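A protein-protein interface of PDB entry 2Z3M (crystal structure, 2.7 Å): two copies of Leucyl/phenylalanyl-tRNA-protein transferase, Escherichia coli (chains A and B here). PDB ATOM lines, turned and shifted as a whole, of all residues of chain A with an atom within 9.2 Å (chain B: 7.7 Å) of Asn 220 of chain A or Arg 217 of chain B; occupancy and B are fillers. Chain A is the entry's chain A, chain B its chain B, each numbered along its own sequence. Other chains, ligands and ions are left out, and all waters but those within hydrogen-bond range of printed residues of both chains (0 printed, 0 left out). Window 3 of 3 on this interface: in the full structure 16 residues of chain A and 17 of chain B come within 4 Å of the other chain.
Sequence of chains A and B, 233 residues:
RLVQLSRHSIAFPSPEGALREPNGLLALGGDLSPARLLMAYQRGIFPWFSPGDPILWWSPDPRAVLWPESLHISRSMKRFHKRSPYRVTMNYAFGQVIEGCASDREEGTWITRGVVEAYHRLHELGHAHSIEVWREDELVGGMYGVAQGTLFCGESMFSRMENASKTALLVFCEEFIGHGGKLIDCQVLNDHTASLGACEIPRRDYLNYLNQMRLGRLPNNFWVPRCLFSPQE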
ATOM      1  N   ASN A  91      30.473  -1.802  14.002  1.00  0.00           N
ATOM      2  CA  ASN A  91      29.593  -2.040  15.139  1.00  0.00           C
ATOM      3  C   ASN A  91      28.115  -2.207  14.768  1.00  0.00           C
ATOM      4  O   ASN A  91      27.243  -1.596  15.373  1.00  0.00           O
ATOM      5  CB  ASN A  91      29.736  -0.910  16.172  1.00  0.00           C
ATOM      6  CG  ASN A  91      31.043  -0.986  16.955  1.00  0.00           C
ATOM      7  OD1 ASN A  91      31.493  -2.068  17.337  1.00  0.00           O
ATOM      8  ND2 ASN A  91      31.646   0.169  17.213  1.00  0.00           N
ATOM      9  N   HIS A 123      31.721  -4.650  24.757  1.00  0.00           N
ATOM     10  CA  HIS A 123      31.093  -3.997  23.623  1.00  0.00           C
ATOM     11  C   HIS A 123      29.974  -3.101  24.136  1.00  0.00           C
ATOM     12  O   HIS A 123      29.730  -2.025  23.600  1.00  0.00           O
ATOM     13  CB  HIS A 123      30.523  -5.029  22.656  1.00  0.00           C
ATOM     14  CG  HIS A 123      29.762  -4.424  21.521  1.00  0.00           C
ATOM     15  ND1 HIS A 123      30.314  -3.489  20.673  1.00  0.00           N
ATOM     16  CD2 HIS A 123      28.497  -4.629  21.085  1.00  0.00           C
ATOM     17  CE1 HIS A 123      29.424  -3.147  19.759  1.00  0.00           C
ATOM     18  NE2 HIS A 123      28.314  -3.826  19.986  1.00  0.00           N
ATOM     19  N   GLU A 124      29.301  -3.564  25.181  1.00  0.00           N
ATOM     20  CA  GLU A 124      28.210  -2.827  25.802  1.00  0.00           C
ATOM     21  C   GLU A 124      28.754  -1.510  26.348  1.00  0.00           C
ATOM     22  O   GLU A 124      28.181  -0.454  26.117  1.00  0.00           O
ATOM     23  CB  GLU A 124      27.620  -3.663  26.935  1.00  0.00           C
ATOM     24  CG  GLU A 124      26.167  -3.381  27.257  1.00  0.00           C
ATOM     25  CD  GLU A 124      25.573  -4.422  28.201  1.00  0.00           C
ATOM     26  OE1 GLU A 124      24.332  -4.463  28.328  1.00  0.00           O
ATOM     27  OE2 GLU A 124      26.341  -5.196  28.817  1.00  0.00           O
ATOM     28  N   LEU A 125      29.877  -1.584  27.052  1.00  0.00           N
ATOM     29  CA  LEU A 125      30.515  -0.409  27.644  1.00  0.00           C
ATOM     30  C   LEU A 125      31.298   0.433  26.638  1.00  0.00           C
ATOM     31  O   LEU A 125      31.888   1.446  27.000  1.00  0.00           O
ATOM     32  CB  LEU A 125      31.440  -0.846  28.787  1.00  0.00           C
ATOM     33  CG  LEU A 125      30.685  -1.651  29.852  1.00  0.00           C
ATOM     34  CD1 LEU A 125      31.631  -2.538  30.638  1.00  0.00           C
ATOM     35  CD2 LEU A 125      29.939  -0.690  30.757  1.00  0.00           C
ATOM     36  N   GLY A 126      31.314   0.007  25.381  1.00  0.00           N
ATOM     37  CA  GLY A 126      32.004   0.765  24.350  1.00  0.00           C
ATOM     38  C   GLY A 126      33.503   0.589  24.166  1.00  0.00           C
ATOM     39  O   GLY A 126      34.140   1.443  23.542  1.00  0.00           O
ATOM     40  N   HIS A 127      34.080  -0.490  24.687  1.00  0.00           N
ATOM     41  CA  HIS A 127      35.516  -0.711  24.524  1.00  0.00           C
ATOM     42  C   HIS A 127      35.826  -1.714  23.415  1.00  0.00           C
ATOM     43  O   HIS A 127      36.851  -1.603  22.743  1.00  0.00           O
ATOM     44  CB  HIS A 127      36.151  -1.212  25.823  1.00  0.00           C
ATOM     45  CG  HIS A 127      36.000  -0.273  26.977  1.00  0.00           C
ATOM     46  ND1 HIS A 127      35.038  -0.439  27.951  1.00  0.00           N
ATOM     47  CD2 HIS A 127      36.687   0.842  27.313  1.00  0.00           C
ATOM     48  CE1 HIS A 127      35.144   0.532  28.839  1.00  0.00           C
ATOM     49  NE2 HIS A 127      36.137   1.322  28.476  1.00  0.00           N
ATOM     50  N   HIS A 129      34.900  -3.502  19.811  1.00  0.00           N
ATOM     51  CA  HIS A 129      34.248  -3.084  18.573  1.00  0.00           C
ATOM     52  C   HIS A 129      34.365  -4.124  17.468  1.00  0.00           C
ATOM     53  O   HIS A 129      35.293  -4.936  17.459  1.00  0.00           O
ATOM     54  CB  HIS A 129      34.871  -1.765  18.087  1.00  0.00           C
ATOM     55  CG  HIS A 129      35.000  -0.735  19.162  1.00  0.00           C
ATOM     56  ND1 HIS A 129      33.950   0.067  19.554  1.00  0.00           N
ATOM     57  CD2 HIS A 129      36.035  -0.423  19.976  1.00  0.00           C
ATOM     58  CE1 HIS A 129      34.332   0.826  20.565  1.00  0.00           C
ATOM     59  NE2 HIS A 129      35.593   0.549  20.841  1.00  0.00           N
ATOM     60  N   HIS A 179      41.866   8.757  11.122  1.00  0.00           N
ATOM     61  CA  HIS A 179      41.586   9.447  12.371  1.00  0.00           C
ATOM     62  C   HIS A 179      42.643   9.309  13.456  1.00  0.00           C
ATOM     63  O   HIS A 179      42.355   9.480  14.645  1.00  0.00           O
ATOM     64  CB  HIS A 179      40.226   9.014  12.900  1.00  0.00           C
ATOM     65  CG  HIS A 179      39.094   9.471  12.041  1.00  0.00           C
ATOM     66  ND1 HIS A 179      38.927   9.037  10.744  1.00  0.00           N
ATOM     67  CD2 HIS A 179      38.103  10.362  12.271  1.00  0.00           C
ATOM     68  CE1 HIS A 179      37.880   9.641  10.212  1.00  0.00           C
ATOM     69  NE2 HIS A 179      37.362  10.450  11.118  1.00  0.00           N
ATOM     70  N   ARG A 217      44.288   9.680  21.846  1.00  0.00           N
ATOM     71  CA  ARG A 217      42.854   9.455  21.675  1.00  0.00           C
ATOM     72  C   ARG A 217      42.375   9.607  20.246  1.00  0.00           C
ATOM     73  O   ARG A 217      43.020  10.265  19.435  1.00  0.00           O
ATOM     74  CB  ARG A 217      42.044  10.396  22.573  1.00  0.00           C
ATOM     75  CG  ARG A 217      41.783   9.855  23.975  1.00  0.00           C
ATOM     76  CD  ARG A 217      40.841  10.763  24.757  1.00  0.00           C
ATOM     77  NE  ARG A 217      39.602  11.033  24.025  1.00  0.00           N
ATOM     78  CZ  ARG A 217      38.600  11.777  24.490  1.00  0.00           C
ATOM     79  NH1 ARG A 217      38.682  12.329  25.693  1.00  0.00           N
ATOM     80  NH2 ARG A 217      37.519  11.978  23.746  1.00  0.00           N
ATOM     81  N   LEU A 218      41.244   8.971  19.948  1.00  0.00           N
ATOM     82  CA  LEU A 218      40.618   9.036  18.626  1.00  0.00           C
ATOM     83  C   LEU A 218      39.385   9.933  18.768  1.00  0.00           C
ATOM     84  O   LEU A 218      38.960  10.238  19.887  1.00  0.00           O
ATOM     85  CB  LEU A 218      40.170   7.642  18.167  1.00  0.00           C
ATOM     86  CG  LEU A 218      41.204   6.567  17.843  1.00  0.00           C
ATOM     87  CD1 LEU A 218      40.491   5.256  17.551  1.00  0.00           C
ATOM     88  CD2 LEU A 218      42.039   6.999  16.648  1.00  0.00           C
ATOM     89  N   PRO A 219      38.788  10.362  17.641  1.00  0.00           N
ATOM     90  CA  PRO A 219      37.606  11.224  17.739  1.00  0.00           C
ATOM     91  C   PRO A 219      36.502  10.618  18.603  1.00  0.00           C
ATOM     92  O   PRO A 219      36.092   9.479  18.395  1.00  0.00           O
ATOM     93  CB  PRO A 219      37.193  11.414  16.280  1.00  0.00           C
ATOM     94  CG  PRO A 219      37.743  10.207  15.596  1.00  0.00           C
ATOM     95  CD  PRO A 219      39.085  10.039  16.236  1.00  0.00           C
ATOM     96  N   ASN A 220      36.038  11.395  19.576  1.00  0.00           N
ATOM     97  CA  ASN A 220      34.999  10.969  20.507  1.00  0.00           C
ATOM     98  C   ASN A 220      33.956   9.991  19.939  1.00  0.00           C
ATOM     99  O   ASN A 220      33.554   9.051  20.626  1.00  0.00           O
ATOM    100  CB  ASN A 220      34.283  12.202  21.078  1.00  0.00           C
ATOM    101  CG  ASN A 220      33.592  11.918  22.407  1.00  0.00           C
ATOM    102  OD1 ASN A 220      34.247  11.660  23.417  1.00  0.00           O
ATOM    103  ND2 ASN A 220      32.262  11.965  22.408  1.00  0.00           N
ATOM    104  N   ASN A 221      33.528  10.199  18.695  1.00  0.00           N
ATOM    105  CA  ASN A 221      32.517   9.330  18.088  1.00  0.00           C
ATOM    106  C   ASN A 221      33.029   8.453  16.939  1.00  0.00           C
ATOM    107  O   ASN A 221      32.272   8.118  16.019  1.00  0.00           O
ATOM    108  CB  ASN A 221      31.364  10.179  17.564  1.00  0.00           C
ATOM    109  CG  ASN A 221      31.790  11.084  16.421  1.00  0.00           C
ATOM    110  OD1 ASN A 221      32.911  10.972  15.911  1.00  0.00           O
ATOM    111  ND2 ASN A 221      30.897  11.980  16.007  1.00  0.00           N
ATOM    112  N   PHE A 222      34.305   8.081  16.986  1.00  0.00           N
ATOM    113  CA  PHE A 222      34.900   7.244  15.940  1.00  0.00           C
ATOM    114  C   PHE A 222      34.197   5.886  15.784  1.00  0.00           C
ATOM    115  O   PHE A 222      34.055   5.381  14.668  1.00  0.00           O
ATOM    116  CB  PHE A 222      36.395   7.020  16.240  1.00  0.00           C
ATOM    117  CG  PHE A 222      37.079   6.079  15.279  1.00  0.00           C
ATOM    118  CD1 PHE A 222      37.295   6.446  13.953  1.00  0.00           C
ATOM    119  CD2 PHE A 222      37.472   4.812  15.691  1.00  0.00           C
ATOM    120  CE1 PHE A 222      37.889   5.564  13.049  1.00  0.00           C
ATOM    121  CE2 PHE A 222      38.067   3.924  14.795  1.00  0.00           C
ATOM    122  CZ  PHE A 222      38.274   4.304  13.468  1.00  0.00           C
ATOM    123  N   TRP A 223      33.737   5.321  16.901  1.00  0.00           N
ATOM    124  CA  TRP A 223      33.093   4.011  16.908  1.00  0.00           C
ATOM    125  C   TRP A 223      31.560   3.924  16.791  1.00  0.00           C
ATOM    126  O   TRP A 223      30.981   2.865  17.047  1.00  0.00           O
ATOM    127  CB  TRP A 223      33.540   3.243  18.157  1.00  0.00           C
ATOM    128  CG  TRP A 223      35.035   3.216  18.341  1.00  0.00           C
ATOM    129  CD1 TRP A 223      35.778   4.026  19.151  1.00  0.00           C
ATOM    130  CD2 TRP A 223      35.968   2.353  17.676  1.00  0.00           C
ATOM    131  NE1 TRP A 223      37.115   3.721  19.035  1.00  0.00           N
ATOM    132  CE2 TRP A 223      37.259   2.699  18.136  1.00  0.00           C
ATOM    133  CE3 TRP A 223      35.839   1.323  16.737  1.00  0.00           C
ATOM    134  CZ2 TRP A 223      38.411   2.052  17.690  1.00  0.00           C
ATOM    135  CZ3 TRP A 223      36.987   0.679  16.292  1.00  0.00           C
ATOM    136  CH2 TRP A 223      38.257   1.046  16.770  1.00  0.00           C
ATOM    137  N   VAL A 224      30.894   5.004  16.398  1.00  0.00           N
ATOM    138  CA  VAL A 224      29.437   4.954  16.284  1.00  0.00           C
ATOM    139  C   VAL A 224      29.018   4.072  15.122  1.00  0.00           C
ATOM    140  O   VAL A 224      29.625   4.102  14.060  1.00  0.00           O
ATOM    141  CB  VAL A 224      28.828   6.355  16.080  1.00  0.00           C
ATOM    142  CG1 VAL A 224      29.091   7.213  17.300  1.00  0.00           C
ATOM    143  CG2 VAL A 224      29.403   6.996  14.835  1.00  0.00           C
ATOM    144  N   PRO A 225      27.967   3.271  15.309  1.00  0.00           N
ATOM    145  CA  PRO A 225      27.519   2.399  14.223  1.00  0.00           C
ATOM    146  C   PRO A 225      27.279   3.140  12.911  1.00  0.00           C
ATOM    147  O   PRO A 225      26.520   4.107  12.860  1.00  0.00           O
ATOM    148  CB  PRO A 225      26.245   1.785  14.791  1.00  0.00           C
ATOM    149  CG  PRO A 225      26.564   1.672  16.242  1.00  0.00           C
ATOM    150  CD  PRO A 225      27.184   3.023  16.533  1.00  0.00           C
ATOM    151  N   GLN B 148      19.824   5.997  18.117  1.00  0.00           N
ATOM    152  CA  GLN B 148      20.601   6.542  17.013  1.00  0.00           C
ATOM    153  C   GLN B 148      21.393   7.712  17.589  1.00  0.00           C
ATOM    154  O   GLN B 148      21.122   8.868  17.285  1.00  0.00           O
ATOM    155  CB  GLN B 148      19.663   7.044  15.915  1.00  0.00           C
ATOM    156  CG  GLN B 148      20.120   6.728  14.502  1.00  0.00           C
ATOM    157  CD  GLN B 148      19.624   5.382  14.037  1.00  0.00           C
ATOM    158  OE1 GLN B 148      20.133   4.819  13.072  1.00  0.00           O
ATOM    159  NE2 GLN B 148      18.616   4.863  14.720  1.00  0.00           N
ATOM    160  N   GLY B 149      22.359   7.411  18.444  1.00  0.00           N
ATOM    161  CA  GLY B 149      23.136   8.473  19.046  1.00  0.00           C
ATOM    162  C   GLY B 149      22.281   9.225  20.049  1.00  0.00           C
ATOM    163  O   GLY B 149      21.813   8.650  21.029  1.00  0.00           O
ATOM    164  N   THR B 150      22.065  10.511  19.811  1.00  0.00           N
ATOM    165  CA  THR B 150      21.258  11.301  20.721  1.00  0.00           C
ATOM    166  C   THR B 150      19.794  11.333  20.277  1.00  0.00           C
ATOM    167  O   THR B 150      18.982  12.109  20.793  1.00  0.00           O
ATOM    168  CB  THR B 150      21.808  12.726  20.840  1.00  0.00           C
ATOM    169  OG1 THR B 150      21.773  13.360  19.562  1.00  0.00           O
ATOM    170  CG2 THR B 150      23.241  12.695  21.329  1.00  0.00           C
ATOM    171  N   LEU B 151      19.462  10.486  19.310  1.00  0.00           N
ATOM    172  CA  LEU B 151      18.091  10.386  18.828  1.00  0.00           C
ATOM    173  C   LEU B 151      17.513   9.022  19.223  1.00  0.00           C
ATOM    174  O   LEU B 151      18.186   7.994  19.099  1.00  0.00           O
ATOM    175  CB  LEU B 151      18.040  10.537  17.303  1.00  0.00           C
ATOM    176  CG  LEU B 151      16.693  10.086  16.719  1.00  0.00           C
ATOM    177  CD1 LEU B 151      15.589  10.951  17.287  1.00  0.00           C
ATOM    178  CD2 LEU B 151      16.707  10.151  15.208  1.00  0.00           C
ATOM    179  N   HIS B 179      21.496  13.163  30.219  1.00  0.00           N
ATOM    180  CA  HIS B 179      22.772  12.670  29.718  1.00  0.00           C
ATOM    181  C   HIS B 179      23.089  13.050  28.281  1.00  0.00           C
ATOM    182  O   HIS B 179      24.013  12.508  27.681  1.00  0.00           O
ATOM    183  CB  HIS B 179      22.851  11.153  29.897  1.00  0.00           C
ATOM    184  CG  HIS B 179      23.115  10.741  31.309  1.00  0.00           C
ATOM    185  ND1 HIS B 179      22.264   9.922  32.020  1.00  0.00           N
ATOM    186  CD2 HIS B 179      24.103  11.094  32.166  1.00  0.00           C
ATOM    187  CE1 HIS B 179      22.714   9.791  33.256  1.00  0.00           C
ATOM    188  NE2 HIS B 179      23.828  10.493  33.370  1.00  0.00           N
ATOM    189  N   GLY B 180      22.321  13.978  27.722  1.00  0.00           N
ATOM    190  CA  GLY B 180      22.592  14.404  26.367  1.00  0.00           C
ATOM    191  C   GLY B 180      21.591  14.030  25.301  1.00  0.00           C
ATOM    192  O   GLY B 180      21.812  14.342  24.136  1.00  0.00           O
ATOM    193  N   GLY B 181      20.505  13.362  25.676  1.00  0.00           N
ATOM    194  CA  GLY B 181      19.499  12.991  24.695  1.00  0.00           C
ATOM    195  C   GLY B 181      19.004  14.233  23.980  1.00  0.00           C
ATOM    196  O   GLY B 181      19.095  15.333  24.516  1.00  0.00           O
ATOM    197  N   GLN B 212      22.557  14.249  11.867  1.00  0.00           N
ATOM    198  CA  GLN B 212      23.291  15.009  12.864  1.00  0.00           C
ATOM    199  C   GLN B 212      23.371  14.237  14.178  1.00  0.00           C
ATOM    200  O   GLN B 212      24.459  14.006  14.713  1.00  0.00           O
ATOM    201  CB  GLN B 212      22.603  16.358  13.099  1.00  0.00           C
ATOM    202  CG  GLN B 212      23.519  17.470  13.580  1.00  0.00           C
ATOM    203  CD  GLN B 212      24.408  18.016  12.479  1.00  0.00           C
ATOM    204  OE1 GLN B 212      25.204  17.295  11.887  1.00  0.00           O
ATOM    205  NE2 GLN B 212      24.272  19.298  12.202  1.00  0.00           N
ATOM    206  N   MET B 213      22.217  13.811  14.684  1.00  0.00           N
ATOM    207  CA  MET B 213      22.164  13.100  15.960  1.00  0.00           C
ATOM    208  C   MET B 213      22.774  11.696  16.063  1.00  0.00           C
ATOM    209  O   MET B 213      23.271  11.329  17.124  1.00  0.00           O
ATOM    210  CB  MET B 213      20.724  13.077  16.470  1.00  0.00           C
ATOM    211  CG  MET B 213      20.217  14.441  16.887  1.00  0.00           C
ATOM    212  SD  MET B 213      18.422  14.535  17.069  1.00  0.00           S
ATOM    213  CE  MET B 213      18.114  16.186  16.571  1.00  0.00           C
ATOM    214  N   ARG B 214      22.757  10.894  15.004  1.00  0.00           N
ATOM    215  CA  ARG B 214      23.343   9.570  15.156  1.00  0.00           C
ATOM    216  C   ARG B 214      24.851   9.619  15.308  1.00  0.00           C
ATOM    217  O   ARG B 214      25.470   8.627  15.697  1.00  0.00           O
ATOM    218  CB  ARG B 214      22.942   8.623  14.015  1.00  0.00           C
ATOM    219  CG  ARG B 214      22.951   9.198  12.636  1.00  0.00           C
ATOM    220  CD  ARG B 214      22.417   8.157  11.657  1.00  0.00           C
ATOM    221  NE  ARG B 214      23.377   7.082  11.437  1.00  0.00           N
ATOM    222  CZ  ARG B 214      24.186   7.013  10.386  1.00  0.00           C
ATOM    223  NH1 ARG B 214      24.147   7.950   9.451  1.00  0.00           N
ATOM    224  NH2 ARG B 214      25.043   6.012  10.283  1.00  0.00           N
ATOM    225  N   LEU B 215      25.437  10.779  15.029  1.00  0.00           N
ATOM    226  CA  LEU B 215      26.878  10.950  15.165  1.00  0.00           C
ATOM    227  C   LEU B 215      27.194  11.382  16.587  1.00  0.00           C
ATOM    228  O   LEU B 215      28.260  11.071  17.112  1.00  0.00           O
ATOM    229  CB  LEU B 215      27.404  11.983  14.167  1.00  0.00           C
ATOM    230  CG  LEU B 215      27.263  11.576  12.692  1.00  0.00           C
ATOM    231  CD1 LEU B 215      27.886  12.656  11.821  1.00  0.00           C
ATOM    232  CD2 LEU B 215      27.919  10.213  12.434  1.00  0.00           C
ATOM    233  N   GLY B 216      26.265  12.102  17.208  1.00  0.00           N
ATOM    234  CA  GLY B 216      26.464  12.523  18.582  1.00  0.00           C
ATOM    235  C   GLY B 216      26.323  11.283  19.449  1.00  0.00           C
ATOM    236  O   GLY B 216      25.957  10.220  18.939  1.00  0.00           O
ATOM    237  N   ARG B 217      26.618  11.387  20.743  1.00  0.00           N
ATOM    238  CA  ARG B 217      26.487  10.217  21.603  1.00  0.00           C
ATOM    239  C   ARG B 217      26.299  10.472  23.096  1.00  0.00           C
ATOM    240  O   ARG B 217      26.424  11.599  23.586  1.00  0.00           O
ATOM    241  CB  ARG B 217      27.664   9.258  21.383  1.00  0.00           C
ATOM    242  CG  ARG B 217      29.024   9.806  21.754  1.00  0.00           C
ATOM    243  CD  ARG B 217      30.098   8.791  21.394  1.00  0.00           C
ATOM    244  NE  ARG B 217      29.994   7.560  22.177  1.00  0.00           N
ATOM    245  CZ  ARG B 217      30.495   7.406  23.399  1.00  0.00           C
ATOM    246  NH1 ARG B 217      31.143   8.411  23.982  1.00  0.00           N
ATOM    247  NH2 ARG B 217      30.349   6.249  24.038  1.00  0.00           N
ATOM    248  N   LEU B 218      25.996   9.384  23.800  1.00  0.00           N
ATOM    249  CA  LEU B 218      25.727   9.380  25.231  1.00  0.00           C
ATOM    250  C   LEU B 218      26.863   8.731  26.021  1.00  0.00           C
ATOM    251  O   LEU B 218      27.846   8.274  25.447  1.00  0.00           O
ATOM    252  CB  LEU B 218      24.430   8.599  25.469  1.00  0.00           C
ATOM    253  CG  LEU B 218      23.291   9.010  24.535  1.00  0.00           C
ATOM    254  CD1 LEU B 218      22.124   8.043  24.661  1.00  0.00           C
ATOM    255  CD2 LEU B 218      22.864  10.435  24.876  1.00  0.00           C
ATOM    256  N   PRO B 219      26.747   8.702  27.358  1.00  0.00           N
ATOM    257  CA  PRO B 219      27.796   8.084  28.167  1.00  0.00           C
ATOM    258  C   PRO B 219      28.021   6.646  27.707  1.00  0.00           C
ATOM    259  O   PRO B 219      27.100   5.991  27.233  1.00  0.00           O
ATOM    260  CB  PRO B 219      27.222   8.155  29.578  1.00  0.00           C
ATOM    261  CG  PRO B 219      26.480   9.443  29.550  1.00  0.00           C
ATOM    262  CD  PRO B 219      25.762   9.384  28.218  1.00  0.00           C
ATOM    263  N   ASN B 220      29.253   6.171  27.852  1.00  0.00           N
ATOM    264  CA  ASN B 220      29.618   4.820  27.453  1.00  0.00           C
ATOM    265  C   ASN B 220      28.685   3.776  28.047  1.00  0.00           C
ATOM    266  O   ASN B 220      28.374   2.765  27.412  1.00  0.00           O
ATOM    267  CB  ASN B 220      31.050   4.519  27.900  1.00  0.00           C
ATOM    268  CG  ASN B 220      32.048   5.533  27.380  1.00  0.00           C
ATOM    269  OD1 ASN B 220      32.230   5.675  26.170  1.00  0.00           O
ATOM    270  ND2 ASN B 220      32.699   6.248  28.293  1.00  0.00           N
ATOM    271  N   ASN B 221      28.229   4.028  29.264  1.00  0.00           N
ATOM    272  CA  ASN B 221      27.367   3.078  29.942  1.00  0.00           C
ATOM    273  C   ASN B 221      25.904   3.494  30.030  1.00  0.00           C
ATOM    274  O   ASN B 221      25.172   2.997  30.881  1.00  0.00           O
ATOM    275  CB  ASN B 221      27.913   2.830  31.345  1.00  0.00           C
ATOM    276  CG  ASN B 221      27.838   4.064  32.221  1.00  0.00           C
ATOM    277  OD1 ASN B 221      28.099   5.180  31.767  1.00  0.00           O
ATOM    278  ND2 ASN B 221      27.487   3.869  33.485  1.00  0.00           N
ATOM    279  N   PHE B 222      25.463   4.381  29.144  1.00  0.00           N
ATOM    280  CA  PHE B 222      24.082   4.836  29.186  1.00  0.00           C
ATOM    281  C   PHE B 222      23.020   3.757  28.966  1.00  0.00           C
ATOM    282  O   PHE B 222      21.985   3.767  29.634  1.00  0.00           O
ATOM    283  CB  PHE B 222      23.847   5.955  28.176  1.00  0.00           C
ATOM    284  CG  PHE B 222      22.457   6.519  28.230  1.00  0.00           C
ATOM    285  CD1 PHE B 222      22.071   7.345  29.278  1.00  0.00           C
ATOM    286  CD2 PHE B 222      21.514   6.171  27.268  1.00  0.00           C
ATOM    287  CE1 PHE B 222      20.765   7.816  29.373  1.00  0.00           C
ATOM    288  CE2 PHE B 222      20.207   6.632  27.346  1.00  0.00           C
ATOM    289  CZ  PHE B 222      19.828   7.458  28.404  1.00  0.00           C
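ND2 of Asn 221 of chain A is in hydrogen-bond range of O of Leu 215 of chain B (3.0 Å). The backbone carbonyl oxygen of Glu 124 of chain A lies close to the backbone carbonyl oxygen of Asn 220 of chain B, at 3.5 Å.
The backbone carbonyl oxygen (O) of Gln 148 of chain B lies close to the backbone NH (N) of Arg 214 of chain B (3.5 Å). The guanidinium group of Arg 217 of chain B lies within hydrogen-bond range of the side-chain amide oxygen of Asn 220 of chain B (2.9 Å). The side-chain amide oxygen (OD1) of Asn 220 of chain A sits at hydrogen-bond distance from the guanidinium group (NH2) of Arg 217 of chain A (3.3 Å).
Among the printed residues, pairs that only touch across the chains: Leu 125 of chain A with Asn 220 of chain B (3.3 Å), Pro 225 of chain A with Arg 214 of chain B (3.5 Å), Asn 220 of chain A with Arg 217 of chain B (3.5 Å) and Val 224 of chain A with Leu 215 of chain B (3.95 Å).
Asn 220 of chain A touches one residue of chain B. Arg 217 of chain B touches just one residue of chain A: Asn 220 (3.5 Å). No residue of chain A comes within 4 Å of Gly 216 of chain B. No residue of chain A comes within 4 Å of Leu 218 of chain B. Of the printed residues of chain B, Pro 225 of chain A touches Arg 214. Printed residues of chain A within 4 Å of Asn 220 of chain B: Glu 124 (3.5 Å) and Leu 125 (3.3 Å). Of the printed residues of chain B, Leu 125 of chain A touches Asn 220 (3.3 Å). Printed residues of chain B within 4 Å of Glu 124 of chain A: Asn 220 (3.5 Å). Of the printed residues of chain A, Leu 215 of chain B touches Asn 221 and Val 224. Gly 180 of chain B touches none of the printed residues of chain A. Asn 221 of chain B touches none of the printed residues of chain A.
Hydrophobic or aromatic side chains of chain A that line the printed part of chain B: Val 224. Along chain A the printed residues that touch a printed residue of chain B span positions 124 to 225. Among the printed residues, 6 pairs touch across the chains.
Asn 220 of chain A touches Arg 217 of chain B, but with the chains exchanged Arg 217 of chain A does not touch Asn 220 of chain B (8.6 Å). Of the 6 pairs that touch across the chains among the printed residues, none has its exchanged pair printed and touching as well.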
